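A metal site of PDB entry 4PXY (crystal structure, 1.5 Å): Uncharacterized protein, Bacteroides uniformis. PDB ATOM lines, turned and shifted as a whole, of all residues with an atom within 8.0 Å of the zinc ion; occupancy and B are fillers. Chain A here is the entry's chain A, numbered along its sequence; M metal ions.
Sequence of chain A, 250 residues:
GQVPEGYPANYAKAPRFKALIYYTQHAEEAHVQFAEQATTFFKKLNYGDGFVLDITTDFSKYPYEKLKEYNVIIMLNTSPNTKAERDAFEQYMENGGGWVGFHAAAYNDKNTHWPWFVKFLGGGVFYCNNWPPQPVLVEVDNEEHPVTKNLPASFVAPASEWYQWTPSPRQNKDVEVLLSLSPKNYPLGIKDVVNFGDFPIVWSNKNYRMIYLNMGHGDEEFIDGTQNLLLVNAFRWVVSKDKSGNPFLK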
ATOM      1  N   GLU A  28      20.531  -7.121  20.161  1.00  0.00           N
ATOM      2  CA  GLU A  28      19.693  -7.081  21.335  1.00  0.00           C
ATOM      3  C   GLU A  28      18.362  -7.731  20.997  1.00  0.00           C
ATOM      4  O   GLU A  28      17.869  -7.666  19.852  1.00  0.00           O
ATOM      5  CB  GLU A  28      19.496  -5.652  21.859  1.00  0.00           C
ATOM      6  CG  GLU A  28      18.706  -4.728  20.989  1.00  0.00           C
ATOM      7  CD  GLU A  28      18.557  -3.355  21.654  1.00  0.00           C
ATOM      8  OE1 GLU A  28      17.628  -3.128  22.484  1.00  0.00           O
ATOM      9  OE2 GLU A  28      19.391  -2.525  21.344  1.00  0.00           O
ATOM     10  N   ALA A  30      15.227  -7.123  21.442  1.00  0.00           N
ATOM     11  CA  ALA A  30      14.150  -6.353  20.784  1.00  0.00           C
ATOM     12  C   ALA A  30      14.341  -6.234  19.261  1.00  0.00           C
ATOM     13  O   ALA A  30      13.393  -6.149  18.511  1.00  0.00           O
ATOM     14  CB  ALA A  30      14.057  -5.003  21.407  1.00  0.00           C
ATOM     15  N   HIS A  31      15.582  -6.227  18.812  1.00  0.00           N
ATOM     16  CA  HIS A  31      15.862  -6.084  17.409  1.00  0.00           C
ATOM     17  C   HIS A  31      15.720  -7.425  16.697  1.00  0.00           C
ATOM     18  O   HIS A  31      15.354  -7.453  15.516  1.00  0.00           O
ATOM     19  CB  HIS A  31      17.263  -5.509  17.219  1.00  0.00           C
ATOM     20  CG  HIS A  31      17.387  -4.114  17.712  1.00  0.00           C
ATOM     21  ND1 HIS A  31      18.541  -3.381  17.603  1.00  0.00           N
ATOM     22  CD2 HIS A  31      16.479  -3.309  18.319  1.00  0.00           C
ATOM     23  CE1 HIS A  31      18.341  -2.188  18.116  1.00  0.00           C
ATOM     24  NE2 HIS A  31      17.129  -2.120  18.601  1.00  0.00           N
ATOM     25  N   PHE A  34      11.739  -7.795  16.478  1.00  0.00           N
ATOM     26  CA  PHE A  34      11.194  -7.051  15.359  1.00  0.00           C
ATOM     27  C   PHE A  34      11.445  -7.772  14.043  1.00  0.00           C
ATOM     28  O   PHE A  34      10.558  -7.920  13.190  1.00  0.00           O
ATOM     29  CB  PHE A  34      11.699  -5.648  15.261  1.00  0.00           C
ATOM     30  CG  PHE A  34      11.285  -4.991  14.004  1.00  0.00           C
ATOM     31  CD1 PHE A  34       9.986  -4.601  13.837  1.00  0.00           C
ATOM     32  CD2 PHE A  34      12.181  -4.763  12.946  1.00  0.00           C
ATOM     33  CE1 PHE A  34       9.571  -3.993  12.654  1.00  0.00           C
ATOM     34  CE2 PHE A  34      11.753  -4.158  11.765  1.00  0.00           C
ATOM     35  CZ  PHE A  34      10.446  -3.783  11.620  1.00  0.00           C
ATOM     36  N   HIS A 103      15.609   0.683  11.176  1.00  0.00           N
ATOM     37  CA  HIS A 103      16.132   0.789  12.548  1.00  0.00           C
ATOM     38  C   HIS A 103      17.642   0.698  12.558  1.00  0.00           C
ATOM     39  O   HIS A 103      18.284   1.502  11.901  1.00  0.00           O
ATOM     40  CB  HIS A 103      15.403  -0.238  13.449  1.00  0.00           C
ATOM     41  CG  HIS A 103      15.392   0.094  14.917  1.00  0.00           C
ATOM     42  ND1 HIS A 103      14.821   1.250  15.396  1.00  0.00           N
ATOM     43  CD2 HIS A 103      15.809  -0.606  15.976  1.00  0.00           C
ATOM     44  CE1 HIS A 103      14.849   1.226  16.714  1.00  0.00           C
ATOM     45  NE2 HIS A 103      15.452   0.110  17.089  1.00  0.00           N
ATOM     46  N   ALA A 104      18.221  -0.248  13.273  1.00  0.00           N
ATOM     47  CA  ALA A 104      19.652  -0.258  13.373  1.00  0.00           C
ATOM     48  C   ALA A 104      20.374  -0.767  12.140  1.00  0.00           C
ATOM     49  O   ALA A 104      21.633  -0.744  12.120  1.00  0.00           O
ATOM     50  CB  ALA A 104      20.125  -1.054  14.573  1.00  0.00           C
ATOM     51  N   ASN A 129      19.363   9.531  20.682  1.00  0.00           N
ATOM     52  CA  ASN A 129      18.071   8.809  20.676  1.00  0.00           C
ATOM     53  C   ASN A 129      17.331   9.076  21.978  1.00  0.00           C
ATOM     54  O   ASN A 129      17.955   9.417  22.984  1.00  0.00           O
ATOM     55  CB  ASN A 129      18.279   7.318  20.498  1.00  0.00           C
ATOM     56  CG  ASN A 129      19.005   6.702  21.663  1.00  0.00           C
ATOM     57  OD1 ASN A 129      20.231   6.894  21.845  1.00  0.00           O
ATOM     58  ND2 ASN A 129      18.261   6.009  22.529  1.00  0.00           N
ATOM     59  N   TRP A 131      14.970   7.424  25.082  1.00  0.00           N
ATOM     60  CA  TRP A 131      14.760   6.152  25.735  1.00  0.00           C
ATOM     61  C   TRP A 131      13.768   6.375  26.880  1.00  0.00           C
ATOM     62  O   TRP A 131      13.882   7.381  27.593  1.00  0.00           O
ATOM     63  CB  TRP A 131      16.057   5.533  26.219  1.00  0.00           C
ATOM     64  CG  TRP A 131      15.863   4.105  26.628  1.00  0.00           C
ATOM     65  CD1 TRP A 131      15.579   3.634  27.866  1.00  0.00           C
ATOM     66  CD2 TRP A 131      15.860   2.972  25.742  1.00  0.00           C
ATOM     67  NE1 TRP A 131      15.397   2.244  27.822  1.00  0.00           N
ATOM     68  CE2 TRP A 131      15.549   1.840  26.509  1.00  0.00           C
ATOM     69  CE3 TRP A 131      16.044   2.817  24.369  1.00  0.00           C
ATOM     70  CZ2 TRP A 131      15.485   0.557  25.927  1.00  0.00           C
ATOM     71  CZ3 TRP A 131      15.955   1.539  23.818  1.00  0.00           C
ATOM     72  CH2 TRP A 131      15.666   0.446  24.583  1.00  0.00           C
ATOM     73  N   PRO A 133      11.633   3.167  24.434  1.00  0.00           N
ATOM     74  CA  PRO A 133      10.723   3.142  23.318  1.00  0.00           C
ATOM     75  C   PRO A 133       9.326   3.611  23.733  1.00  0.00           C
ATOM     76  O   PRO A 133       8.807   3.249  24.773  1.00  0.00           O
ATOM     77  CB  PRO A 133      10.713   1.648  22.924  1.00  0.00           C
ATOM     78  CG  PRO A 133      12.024   1.166  23.328  1.00  0.00           C
ATOM     79  CD  PRO A 133      12.349   1.895  24.617  1.00  0.00           C
ATOM     80  N   SER A 160       8.780   2.809  19.512  1.00  0.00           N
ATOM     81  CA  SER A 160      10.140   2.497  19.128  1.00  0.00           C
ATOM     82  C   SER A 160      10.997   3.502  19.887  1.00  0.00           C
ATOM     83  O   SER A 160      10.503   4.546  20.397  1.00  0.00           O
ATOM     84  CB  SER A 160      10.303   2.610  17.610  1.00  0.00           C
ATOM     85  OG  SER A 160      11.606   2.155  17.206  1.00  0.00           O
ATOM     86  N   GLU A 161      12.303   3.243  19.932  1.00  0.00           N
ATOM     87  CA  GLU A 161      13.247   4.297  20.218  1.00  0.00           C
ATOM     88  C   GLU A 161      13.660   4.892  18.879  1.00  0.00           C
ATOM     89  O   GLU A 161      13.570   4.204  17.864  1.00  0.00           O
ATOM     90  CB  GLU A 161      14.464   3.962  21.091  1.00  0.00           C
ATOM     91  CG  GLU A 161      15.684   3.323  20.433  1.00  0.00           C
ATOM     92  CD  GLU A 161      15.478   1.881  20.013  1.00  0.00           C
ATOM     93  OE1 GLU A 161      14.320   1.459  19.734  1.00  0.00           O
ATOM     94  OE2 GLU A 161      16.518   1.175  19.951  1.00  0.00           O
ATOM     95  N   TRP A 162      13.834   6.199  18.881  1.00  0.00           N
ATOM     96  CA  TRP A 162      13.967   6.988  17.680  1.00  0.00           C
ATOM     97  C   TRP A 162      15.326   7.683  17.629  1.00  0.00           C
ATOM     98  O   TRP A 162      15.817   8.129  18.650  1.00  0.00           O
ATOM     99  CB  TRP A 162      12.844   7.999  17.618  1.00  0.00           C
ATOM    100  CG  TRP A 162      11.470   7.375  17.749  1.00  0.00           C
ATOM    101  CD1 TRP A 162      10.723   7.309  18.873  1.00  0.00           C
ATOM    102  CD2 TRP A 162      10.698   6.776  16.709  1.00  0.00           C
ATOM    103  NE1 TRP A 162       9.527   6.677  18.615  1.00  0.00           N
ATOM    104  CE2 TRP A 162       9.496   6.317  17.300  1.00  0.00           C
ATOM    105  CE3 TRP A 162      10.935   6.512  15.361  1.00  0.00           C
ATOM    106  CZ2 TRP A 162       8.537   5.677  16.586  1.00  0.00           C
ATOM    107  CZ3 TRP A 162       9.950   5.924  14.627  1.00  0.00           C
ATOM    108  CH2 TRP A 162       8.764   5.478  15.243  1.00  0.00           C
ATOM    109  N   TYR A 163      15.944   7.686  16.451  1.00  0.00           N
ATOM    110  CA  TYR A 163      17.290   8.220  16.275  1.00  0.00           C
ATOM    111  C   TYR A 163      17.319   9.578  15.588  1.00  0.00           C
ATOM    112  O   TYR A 163      16.666   9.765  14.576  1.00  0.00           O
ATOM    113  CB  TYR A 163      18.114   7.278  15.363  1.00  0.00           C
ATOM    114  CG  TYR A 163      18.392   5.872  15.788  1.00  0.00           C
ATOM    115  CD1 TYR A 163      18.015   5.340  17.014  1.00  0.00           C
ATOM    116  CD2 TYR A 163      19.017   5.020  14.866  1.00  0.00           C
ATOM    117  CE1 TYR A 163      18.281   4.004  17.312  1.00  0.00           C
ATOM    118  CE2 TYR A 163      19.287   3.691  15.153  1.00  0.00           C
ATOM    119  CZ  TYR A 163      18.884   3.197  16.351  1.00  0.00           C
ATOM    120  OH  TYR A 163      19.212   1.860  16.582  1.00  0.00           O
ATOM    121  N   ASN A 214      13.018   4.355  10.304  1.00  0.00           N
ATOM    122  CA  ASN A 214      13.780   4.325  11.571  1.00  0.00           C
ATOM    123  C   ASN A 214      13.180   3.343  12.595  1.00  0.00           C
ATOM    124  O   ASN A 214      13.868   2.903  13.500  1.00  0.00           O
ATOM    125  CB  ASN A 214      13.879   5.728  12.184  1.00  0.00           C
ATOM    126  CG  ASN A 214      14.766   5.823  13.412  1.00  0.00           C
ATOM    127  OD1 ASN A 214      14.386   6.486  14.373  1.00  0.00           O
ATOM    128  ND2 ASN A 214      15.969   5.298  13.345  1.00  0.00           N
ATOM    129  N   MET A 215      11.904   3.099  12.538  1.00  0.00           N
ATOM    130  CA  MET A 215      11.279   2.198  13.501  1.00  0.00           C
ATOM    131  C   MET A 215      11.726   0.767  13.299  1.00  0.00           C
ATOM    132  O   MET A 215      12.123   0.358  12.187  1.00  0.00           O
ATOM    133  CB  MET A 215       9.762   2.344  13.553  1.00  0.00           C
ATOM    134  CG  MET A 215       9.044   1.716  12.459  1.00  0.00           C
ATOM    135  SD  MET A 215       8.983   2.887  10.860  1.00  0.00           S
ATOM    136  CE  MET A 215       7.790   4.292  11.579  1.00  0.00           C
ATOM    137  N   GLY A 216      11.644  -0.035  14.348  1.00  0.00           N
ATOM    138  CA  GLY A 216      11.795  -1.493  14.261  1.00  0.00           C
ATOM    139  C   GLY A 216      12.344  -2.063  15.546  1.00  0.00           C
ATOM    140  O   GLY A 216      13.374  -2.735  15.548  1.00  0.00           O
ATOM    141  N   HIS A 217      11.612  -1.902  16.653  1.00  0.00           N
ATOM    142  CA  HIS A 217      12.081  -2.316  17.936  1.00  0.00           C
ATOM    143  C   HIS A 217      11.025  -3.119  18.684  1.00  0.00           C
ATOM    144  O   HIS A 217       9.962  -2.552  19.028  1.00  0.00           O
ATOM    145  CB  HIS A 217      12.432  -1.068  18.758  1.00  0.00           C
ATOM    146  CG  HIS A 217      13.092  -1.364  20.082  1.00  0.00           C
ATOM    147  ND1 HIS A 217      14.457  -1.370  20.232  1.00  0.00           N
ATOM    148  CD2 HIS A 217      12.594  -1.716  21.307  1.00  0.00           C
ATOM    149  CE1 HIS A 217      14.777  -1.666  21.488  1.00  0.00           C
ATOM    150  NE2 HIS A 217      13.662  -1.887  22.158  1.00  0.00           N
ATOM    151  N   GLY A 218      11.314  -4.350  19.099  1.00  0.00           N
ATOM    152  CA  GLY A 218      10.422  -5.102  19.934  1.00  0.00           C
ATOM    153  C   GLY A 218       9.355  -5.924  19.242  1.00  0.00           C
ATOM    154  O   GLY A 218       9.436  -6.135  18.018  1.00  0.00           O
ATOM    155  N   GLU A 221       5.392  -3.908  17.105  1.00  0.00           N
ATOM    156  CA  GLU A 221       5.439  -2.874  16.050  1.00  0.00           C
ATOM    157  C   GLU A 221       4.297  -2.992  15.009  1.00  0.00           C
ATOM    158  O   GLU A 221       4.165  -2.094  14.172  1.00  0.00           O
ATOM    159  CB  GLU A 221       6.765  -2.902  15.285  1.00  0.00           C
ATOM    160  CG  GLU A 221       7.979  -2.386  16.088  1.00  0.00           C
ATOM    161  CD  GLU A 221       8.121  -0.886  16.014  1.00  0.00           C
ATOM    162  OE1 GLU A 221       7.073  -0.190  15.798  1.00  0.00           O
ATOM    163  OE2 GLU A 221       9.238  -0.371  16.190  1.00  0.00           O
HETATM  164 ZN    ZN M   1      15.854  -0.514  19.008  1.00  0.00          ZN
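The zinc ion is bound by the side-chain carboxylate (OE2) of Glu 161 (2.0 Å). ND1 of His 217 binds the zinc ion (2.0 Å). A ring nitrogen (NE2) of His 103 binds the zinc ion, 2.1 Å away. NE2 of His 31 binds the zinc ion. Slightly farther from the zinc ion lies OE1 of Glu 161 (2.6 Å).
Of the 19 residues printed, 4 come within 4 Å of the zinc ion. The nearest printed residue that does not touch the zinc ion is Glu 28 (4.7 Å).
The backbone NH (N) of His 217 sits at hydrogen-bond distance from the side-chain carboxylate (OE2) of Glu 221, at 2.9 Å. ND1 of His 103 lies within hydrogen-bond range of O of Asn 214 (2.7 Å).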
